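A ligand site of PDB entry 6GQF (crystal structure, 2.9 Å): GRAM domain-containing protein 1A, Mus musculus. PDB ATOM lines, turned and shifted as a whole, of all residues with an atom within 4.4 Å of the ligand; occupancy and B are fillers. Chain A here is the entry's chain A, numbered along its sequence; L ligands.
OH of Tyr 96 sits close to O1 of the ligand, 3.4 Å away. The side-chain amide oxygen (OD1) of Asn 102 sits at hydrogen-bond distance from an oxygen (O2) of the ligand. The side-chain hydroxyl (OH) of Tyr 193 lies within hydrogen-bond range of an oxygen (O1) of the ligand, at 3.3 Å. The side-chain amide oxygen (OD1) of Asn 185 lies within hydrogen-bond range of an oxygen (O2) of the ligand.
Merely in contact with the ligand: Ile 98, Leu 104, Val 133, Thr 135, Pro 139, Phe 144, Thr 146, His 148, Ser 186 and Gly 189. Hydrophobic or aromatic side chains within 4 Å of the ligand: Tyr 96, Ile 98, Leu 104, Val 133, Pro 139, Phe 144, His 148 and Tyr 193. Within 4 Å of the ligand: Tyr 96, Ile 98, Asn 102, Leu 104, Val 133, Thr 135, Pro 139, Phe 144, Thr 146, His 148, Asn 185, Ser 186, Gly 189 and Tyr 193. Along chain A the residues within 4 Å of the ligand span positions 96 to 193.
The side-chain hydroxyl of Tyr 96 lies within hydrogen-bond range of the side-chain carboxylate of Glu 113 (2.7 Å). OG1 of Thr 146 lies within hydrogen-bond range of NE2 of His 148 (2.9 Å). O of Thr 146 sits at hydrogen-bond distance from N of Val 133 (3.1 Å). OG of Ser 186 is in hydrogen-bond range of O of Ile 182, at 2.7 Å. The side-chain amide oxygen (OD1) of Asn 185 sits close to the backbone carbonyl oxygen (O) of Leu 181 (2.8 Å).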
ATOM      1  N   PHE A  74     -34.237  24.544  12.068  1.00  0.00           N
ATOM      2  CA  PHE A  74     -33.042  25.281  11.697  1.00  0.00           C
ATOM      3  C   PHE A  74     -33.412  26.676  11.218  1.00  0.00           C
ATOM      4  O   PHE A  74     -34.283  26.827  10.361  1.00  0.00           O
ATOM      5  CB  PHE A  74     -32.266  24.534  10.609  1.00  0.00           C
ATOM      6  CG  PHE A  74     -31.647  23.243  11.073  1.00  0.00           C
ATOM      7  CD1 PHE A  74     -31.733  22.834  12.397  1.00  0.00           C
ATOM      8  CD2 PHE A  74     -30.983  22.437  10.172  1.00  0.00           C
ATOM      9  CE1 PHE A  74     -31.160  21.644  12.809  1.00  0.00           C
ATOM     10  CE2 PHE A  74     -30.411  21.248  10.570  1.00  0.00           C
ATOM     11  CZ  PHE A  74     -30.500  20.852  11.888  1.00  0.00           C
ATOM     12  N   TYR A  96     -26.428  27.742   8.756  1.00  0.00           N
ATOM     13  CA  TYR A  96     -27.692  27.760   9.478  1.00  0.00           C
ATOM     14  C   TYR A  96     -27.447  27.611  10.965  1.00  0.00           C
ATOM     15  O   TYR A  96     -26.429  27.063  11.380  1.00  0.00           O
ATOM     16  CB  TYR A  96     -28.635  26.668   8.975  1.00  0.00           C
ATOM     17  CG  TYR A  96     -27.938  25.368   8.647  1.00  0.00           C
ATOM     18  CD1 TYR A  96     -27.427  24.559   9.648  1.00  0.00           C
ATOM     19  CD2 TYR A  96     -27.796  24.960   7.329  1.00  0.00           C
ATOM     20  CE1 TYR A  96     -26.774  23.373   9.347  1.00  0.00           C
ATOM     21  CE2 TYR A  96     -27.160  23.771   7.014  1.00  0.00           C
ATOM     22  CZ  TYR A  96     -26.654  22.984   8.031  1.00  0.00           C
ATOM     23  OH  TYR A  96     -26.021  21.808   7.711  1.00  0.00           O
ATOM     24  N   ILE A  98     -28.637  26.047  14.556  1.00  0.00           N
ATOM     25  CA  ILE A  98     -29.297  24.830  15.016  1.00  0.00           C
ATOM     26  C   ILE A  98     -29.565  24.903  16.515  1.00  0.00           C
ATOM     27  O   ILE A  98     -28.914  25.661  17.230  1.00  0.00           O
ATOM     28  CB  ILE A  98     -28.451  23.573  14.726  1.00  0.00           C
ATOM     29  CG1 ILE A  98     -27.155  23.586  15.557  1.00  0.00           C
ATOM     30  CG2 ILE A  98     -28.161  23.458  13.229  1.00  0.00           C
ATOM     31  CD1 ILE A  98     -26.302  22.349  15.375  1.00  0.00           C
ATOM     32  N   ILE A 100     -29.417  23.125  20.293  1.00  0.00           N
ATOM     33  CA  ILE A 100     -28.652  22.147  21.058  1.00  0.00           C
ATOM     34  C   ILE A 100     -29.495  21.685  22.240  1.00  0.00           C
ATOM     35  O   ILE A 100     -30.018  22.500  23.004  1.00  0.00           O
ATOM     36  CB  ILE A 100     -27.297  22.711  21.554  1.00  0.00           C
ATOM     37  CG1 ILE A 100     -26.244  22.666  20.442  1.00  0.00           C
ATOM     38  CG2 ILE A 100     -26.757  21.925  22.749  1.00  0.00           C
ATOM     39  CD1 ILE A 100     -26.482  23.604  19.308  1.00  0.00           C
ATOM     40  N   ASN A 102     -28.510  18.603  24.252  1.00  0.00           N
ATOM     41  CA  ASN A 102     -27.632  18.031  25.277  1.00  0.00           C
ATOM     42  C   ASN A 102     -27.242  19.094  26.307  1.00  0.00           C
ATOM     43  O   ASN A 102     -26.633  20.115  25.962  1.00  0.00           O
ATOM     44  CB  ASN A 102     -26.373  17.385  24.660  1.00  0.00           C
ATOM     45  CG  ASN A 102     -25.851  18.136  23.435  1.00  0.00           C
ATOM     46  OD1 ASN A 102     -25.070  19.093  23.565  1.00  0.00           O
ATOM     47  ND2 ASN A 102     -26.225  17.679  22.249  1.00  0.00           N
ATOM     48  N   LEU A 104     -25.392  20.906  27.836  1.00  0.00           N
ATOM     49  CA  LEU A 104     -23.976  21.266  27.834  1.00  0.00           C
ATOM     50  C   LEU A 104     -23.782  22.584  27.094  1.00  0.00           C
ATOM     51  O   LEU A 104     -23.865  22.640  25.865  1.00  0.00           O
ATOM     52  CB  LEU A 104     -23.144  20.159  27.183  1.00  0.00           C
ATOM     53  CG  LEU A 104     -21.692  20.067  27.651  1.00  0.00           C
ATOM     54  CD1 LEU A 104     -21.610  19.494  29.054  1.00  0.00           C
ATOM     55  CD2 LEU A 104     -20.898  19.213  26.686  1.00  0.00           C
ATOM     56  N   GLU A 113     -21.378  24.841   6.381  1.00  0.00           N
ATOM     57  CA  GLU A 113     -21.199  23.587   5.662  1.00  0.00           C
ATOM     58  C   GLU A 113     -20.696  23.833   4.242  1.00  0.00           C
ATOM     59  O   GLU A 113     -21.084  24.795   3.604  1.00  0.00           O
ATOM     60  CB  GLU A 113     -22.516  22.799   5.632  1.00  0.00           C
ATOM     61  CG  GLU A 113     -22.416  21.421   4.959  1.00  0.00           C
ATOM     62  CD  GLU A 113     -23.738  20.677   4.940  1.00  0.00           C
ATOM     63  OE1 GLU A 113     -24.758  21.265   5.362  1.00  0.00           O
ATOM     64  OE2 GLU A 113     -23.765  19.514   4.505  1.00  0.00           O
ATOM     65  N   VAL A 133     -18.763  19.760   7.597  1.00  0.00           N
ATOM     66  CA  VAL A 133     -19.652  20.462   8.519  1.00  0.00           C
ATOM     67  C   VAL A 133     -18.868  20.966   9.710  1.00  0.00           C
ATOM     68  O   VAL A 133     -18.320  20.185  10.492  1.00  0.00           O
ATOM     69  CB  VAL A 133     -20.806  19.567   8.993  1.00  0.00           C
ATOM     70  CG1 VAL A 133     -21.664  20.289  10.031  1.00  0.00           C
ATOM     71  CG2 VAL A 133     -21.659  19.134   7.818  1.00  0.00           C
ATOM     72  N   THR A 135     -19.353  23.102  13.044  1.00  0.00           N
ATOM     73  CA  THR A 135     -20.274  23.658  14.030  1.00  0.00           C
ATOM     74  C   THR A 135     -19.521  24.639  14.923  1.00  0.00           C
ATOM     75  O   THR A 135     -18.516  24.271  15.548  1.00  0.00           O
ATOM     76  CB  THR A 135     -20.902  22.553  14.878  1.00  0.00           C
ATOM     77  OG1 THR A 135     -19.902  21.939  15.698  1.00  0.00           O
ATOM     78  CG2 THR A 135     -21.523  21.484  13.987  1.00  0.00           C
ATOM     79  N   ILE A 138     -20.093  26.027  19.937  1.00  0.00           N
ATOM     80  CA  ILE A 138     -20.257  24.937  20.885  1.00  0.00           C
ATOM     81  C   ILE A 138     -18.989  24.756  21.703  1.00  0.00           C
ATOM     82  O   ILE A 138     -17.933  25.278  21.347  1.00  0.00           O
ATOM     83  CB  ILE A 138     -20.593  23.603  20.174  1.00  0.00           C
ATOM     84  CG1 ILE A 138     -19.457  23.192  19.228  1.00  0.00           C
ATOM     85  CG2 ILE A 138     -21.903  23.729  19.429  1.00  0.00           C
ATOM     86  CD1 ILE A 138     -19.585  21.775  18.704  1.00  0.00           C
ATOM     87  N   PRO A 139     -19.083  24.002  22.813  1.00  0.00           N
ATOM     88  CA  PRO A 139     -17.895  23.558  23.548  1.00  0.00           C
ATOM     89  C   PRO A 139     -17.013  22.621  22.722  1.00  0.00           C
ATOM     90  O   PRO A 139     -17.523  21.736  22.040  1.00  0.00           O
ATOM     91  CB  PRO A 139     -18.482  22.804  24.745  1.00  0.00           C
ATOM     92  CG  PRO A 139     -19.853  23.356  24.899  1.00  0.00           C
ATOM     93  CD  PRO A 139     -20.327  23.675  23.533  1.00  0.00           C
ATOM     94  N   TYR A 140     -15.699  22.833  22.777  1.00  0.00           N
ATOM     95  CA  TYR A 140     -14.732  21.965  22.113  1.00  0.00           C
ATOM     96  C   TYR A 140     -14.853  22.012  20.584  1.00  0.00           C
ATOM     97  O   TYR A 140     -14.542  21.037  19.907  1.00  0.00           O
ATOM     98  CB  TYR A 140     -14.889  20.516  22.596  1.00  0.00           C
ATOM     99  CG  TYR A 140     -14.877  20.375  24.096  1.00  0.00           C
ATOM    100  CD1 TYR A 140     -13.723  20.619  24.826  1.00  0.00           C
ATOM    101  CD2 TYR A 140     -16.013  19.963  24.784  1.00  0.00           C
ATOM    102  CE1 TYR A 140     -13.700  20.487  26.198  1.00  0.00           C
ATOM    103  CE2 TYR A 140     -16.000  19.823  26.163  1.00  0.00           C
ATOM    104  CZ  TYR A 140     -14.839  20.089  26.867  1.00  0.00           C
ATOM    105  OH  TYR A 140     -14.823  19.958  28.246  1.00  0.00           O
ATOM    106  N   PHE A 144     -12.636  19.386  16.946  1.00  0.00           N
ATOM    107  CA  PHE A 144     -13.143  18.467  15.926  1.00  0.00           C
ATOM    108  C   PHE A 144     -14.065  19.132  14.918  1.00  0.00           C
ATOM    109  O   PHE A 144     -14.557  20.238  15.136  1.00  0.00           O
ATOM    110  CB  PHE A 144     -13.894  17.310  16.601  1.00  0.00           C
ATOM    111  CG  PHE A 144     -15.280  17.685  17.085  1.00  0.00           C
ATOM    112  CD1 PHE A 144     -15.452  18.461  18.215  1.00  0.00           C
ATOM    113  CD2 PHE A 144     -16.409  17.252  16.399  1.00  0.00           C
ATOM    114  CE1 PHE A 144     -16.724  18.802  18.659  1.00  0.00           C
ATOM    115  CE2 PHE A 144     -17.674  17.592  16.835  1.00  0.00           C
ATOM    116  CZ  PHE A 144     -17.830  18.371  17.965  1.00  0.00           C
ATOM    117  N   THR A 146     -16.773  17.391  11.407  1.00  0.00           N
ATOM    118  CA  THR A 146     -17.302  16.118  10.877  1.00  0.00           C
ATOM    119  C   THR A 146     -17.384  16.127   9.351  1.00  0.00           C
ATOM    120  O   THR A 146     -17.557  17.182   8.740  1.00  0.00           O
ATOM    121  CB  THR A 146     -18.700  15.793  11.452  1.00  0.00           C
ATOM    122  OG1 THR A 146     -19.671  16.758  11.023  1.00  0.00           O
ATOM    123  CG2 THR A 146     -18.652  15.755  12.969  1.00  0.00           C
ATOM    124  N   HIS A 148     -19.098  13.953   5.839  1.00  0.00           N
ATOM    125  CA  HIS A 148     -20.208  13.119   5.395  1.00  0.00           C
ATOM    126  C   HIS A 148     -20.165  12.945   3.875  1.00  0.00           C
ATOM    127  O   HIS A 148     -19.853  13.877   3.136  1.00  0.00           O
ATOM    128  CB  HIS A 148     -21.536  13.735   5.825  1.00  0.00           C
ATOM    129  CG  HIS A 148     -21.562  14.150   7.256  1.00  0.00           C
ATOM    130  ND1 HIS A 148     -22.169  13.413   8.242  1.00  0.00           N
ATOM    131  CD2 HIS A 148     -21.014  15.231   7.879  1.00  0.00           C
ATOM    132  CE1 HIS A 148     -22.016  14.008   9.404  1.00  0.00           C
ATOM    133  NE2 HIS A 148     -21.309  15.114   9.216  1.00  0.00           N
ATOM    134  N   LEU A 181     -17.373  12.110  25.283  1.00  0.00           N
ATOM    135  CA  LEU A 181     -18.525  13.002  25.256  1.00  0.00           C
ATOM    136  C   LEU A 181     -18.781  13.560  23.855  1.00  0.00           C
ATOM    137  O   LEU A 181     -19.929  13.696  23.435  1.00  0.00           O
ATOM    138  CB  LEU A 181     -18.319  14.146  26.241  1.00  0.00           C
ATOM    139  CG  LEU A 181     -19.517  15.076  26.474  1.00  0.00           C
ATOM    140  CD1 LEU A 181     -20.709  14.320  27.028  1.00  0.00           C
ATOM    141  CD2 LEU A 181     -19.125  16.215  27.391  1.00  0.00           C
ATOM    142  N   ILE A 182     -17.714  13.885  23.130  1.00  0.00           N
ATOM    143  CA  ILE A 182     -17.846  14.367  21.761  1.00  0.00           C
ATOM    144  C   ILE A 182     -18.382  13.266  20.844  1.00  0.00           C
ATOM    145  O   ILE A 182     -19.241  13.519  19.997  1.00  0.00           O
ATOM    146  CB  ILE A 182     -16.510  14.911  21.210  1.00  0.00           C
ATOM    147  CG1 ILE A 182     -16.023  16.069  22.084  1.00  0.00           C
ATOM    148  CG2 ILE A 182     -16.679  15.372  19.762  1.00  0.00           C
ATOM    149  CD1 ILE A 182     -14.727  16.706  21.637  1.00  0.00           C
ATOM    150  N   ASN A 185     -22.357  12.618  21.958  1.00  0.00           N
ATOM    151  CA  ASN A 185     -23.296  13.676  21.560  1.00  0.00           C
ATOM    152  C   ASN A 185     -23.354  13.890  20.055  1.00  0.00           C
ATOM    153  O   ASN A 185     -24.421  14.168  19.507  1.00  0.00           O
ATOM    154  CB  ASN A 185     -22.928  15.001  22.234  1.00  0.00           C
ATOM    155  CG  ASN A 185     -22.880  14.909  23.752  1.00  0.00           C
ATOM    156  OD1 ASN A 185     -21.966  15.425  24.380  1.00  0.00           O
ATOM    157  ND2 ASN A 185     -23.876  14.253  24.341  1.00  0.00           N
ATOM    158  N   SER A 186     -22.210  13.775  19.389  1.00  0.00           N
ATOM    159  CA  SER A 186     -22.135  13.951  17.941  1.00  0.00           C
ATOM    160  C   SER A 186     -22.924  12.860  17.208  1.00  0.00           C
ATOM    161  O   SER A 186     -23.773  13.174  16.368  1.00  0.00           O
ATOM    162  CB  SER A 186     -20.685  13.941  17.459  1.00  0.00           C
ATOM    163  OG  SER A 186     -19.971  15.078  17.928  1.00  0.00           O
ATOM    164  N   GLY A 189     -26.715  13.188  17.568  1.00  0.00           N
ATOM    165  CA  GLY A 189     -27.250  14.252  16.737  1.00  0.00           C
ATOM    166  C   GLY A 189     -27.125  13.976  15.248  1.00  0.00           C
ATOM    167  O   GLY A 189     -27.909  14.498  14.450  1.00  0.00           O
ATOM    168  N   ILE A 190     -26.142  13.161  14.867  1.00  0.00           N
ATOM    169  CA  ILE A 190     -25.936  12.788  13.472  1.00  0.00           C
ATOM    170  C   ILE A 190     -26.962  11.745  13.033  1.00  0.00           C
ATOM    171  O   ILE A 190     -27.553  11.845  11.959  1.00  0.00           O
ATOM    172  CB  ILE A 190     -24.505  12.263  13.227  1.00  0.00           C
ATOM    173  CG1 ILE A 190     -23.504  13.423  13.239  1.00  0.00           C
ATOM    174  CG2 ILE A 190     -24.389  11.532  11.875  1.00  0.00           C
ATOM    175  CD1 ILE A 190     -22.051  12.999  13.310  1.00  0.00           C
ATOM    176  N   TYR A 193     -30.502  13.132  12.945  1.00  0.00           N
ATOM    177  CA  TYR A 193     -30.714  13.985  11.787  1.00  0.00           C
ATOM    178  C   TYR A 193     -30.987  13.167  10.526  1.00  0.00           C
ATOM    179  O   TYR A 193     -31.998  13.379   9.856  1.00  0.00           O
ATOM    180  CB  TYR A 193     -29.493  14.893  11.555  1.00  0.00           C
ATOM    181  CG  TYR A 193     -29.592  15.690  10.268  1.00  0.00           C
ATOM    182  CD1 TYR A 193     -30.246  16.920  10.246  1.00  0.00           C
ATOM    183  CD2 TYR A 193     -29.066  15.208   9.084  1.00  0.00           C
ATOM    184  CE1 TYR A 193     -30.352  17.644   9.066  1.00  0.00           C
ATOM    185  CE2 TYR A 193     -29.175  15.923   7.903  1.00  0.00           C
ATOM    186  CZ  TYR A 193     -29.816  17.144   7.908  1.00  0.00           C
ATOM    187  OH  TYR A 193     -29.926  17.858   6.741  1.00  0.00           O
HETATM  188  C1  LIG L   1     -24.574  17.118  16.108  1.00  0.00           C
HETATM  189  C2  LIG L   1     -23.777  18.377  15.742  1.00  0.00           C
HETATM  190  C3  LIG L   1     -24.779  19.346  15.408  1.00  0.00           C
HETATM  191  C4  LIG L   1     -25.600  18.983  14.041  1.00  0.00           C
HETATM  192  C5  LIG L   1     -24.694  18.702  12.849  1.00  0.00           C
HETATM  193  C6  LIG L   1     -25.500  18.354  11.491  1.00  0.00           C
HETATM  194  C7  LIG L   1     -26.630  17.406  11.852  1.00  0.00           C
HETATM  195  C8  LIG L   1     -26.145  19.631  10.940  1.00  0.00           C
HETATM  196  C9  LIG L   1     -26.872  19.397   9.634  1.00  0.00           C
HETATM  197  C10 LIG L   1     -25.988  18.774   8.593  1.00  0.00           C
HETATM  198  O1  LIG L   1     -26.762  18.459   7.429  1.00  0.00           O
HETATM  199  C11 LIG L   1     -25.325  17.494   9.093  1.00  0.00           C
HETATM  200  C12 LIG L   1     -24.664  17.729  10.449  1.00  0.00           C
HETATM  201  C13 LIG L   1     -23.394  16.778  10.916  1.00  0.00           C
HETATM  202  C14 LIG L   1     -22.620  17.245  12.082  1.00  0.00           C
HETATM  203  C15 LIG L   1     -23.685  17.627  13.244  1.00  0.00           C
HETATM  204  C16 LIG L   1     -22.928  18.040  14.489  1.00  0.00           C
HETATM  205  C17 LIG L   1     -21.723  17.109  15.016  1.00  0.00           C
HETATM  206  C18 LIG L   1     -21.546  17.615  16.652  1.00  0.00           C
HETATM  207  C19 LIG L   1     -22.665  18.637  16.930  1.00  0.00           C
HETATM  208  C20 LIG L   1     -23.252  18.609  18.260  1.00  0.00           C
HETATM  209  C21 LIG L   1     -23.660  20.069  18.621  1.00  0.00           C
HETATM  210  C22 LIG L   1     -22.394  17.989  19.417  1.00  0.00           C
HETATM  211  C23 LIG L   1     -21.909  18.945  20.476  1.00  0.00           C
HETATM  212  C24 LIG L   1     -20.900  18.166  21.278  1.00  0.00           C
HETATM  213  C25 LIG L   1     -20.672  18.821  22.623  1.00  0.00           C
HETATM  214  C26 LIG L   1     -19.558  18.076  23.306  1.00  0.00           C
HETATM  215  C27 LIG L   1     -20.276  20.275  22.413  1.00  0.00           C
HETATM  216  O2  LIG L   1     -21.854  18.735  23.390  1.00  0.00           O
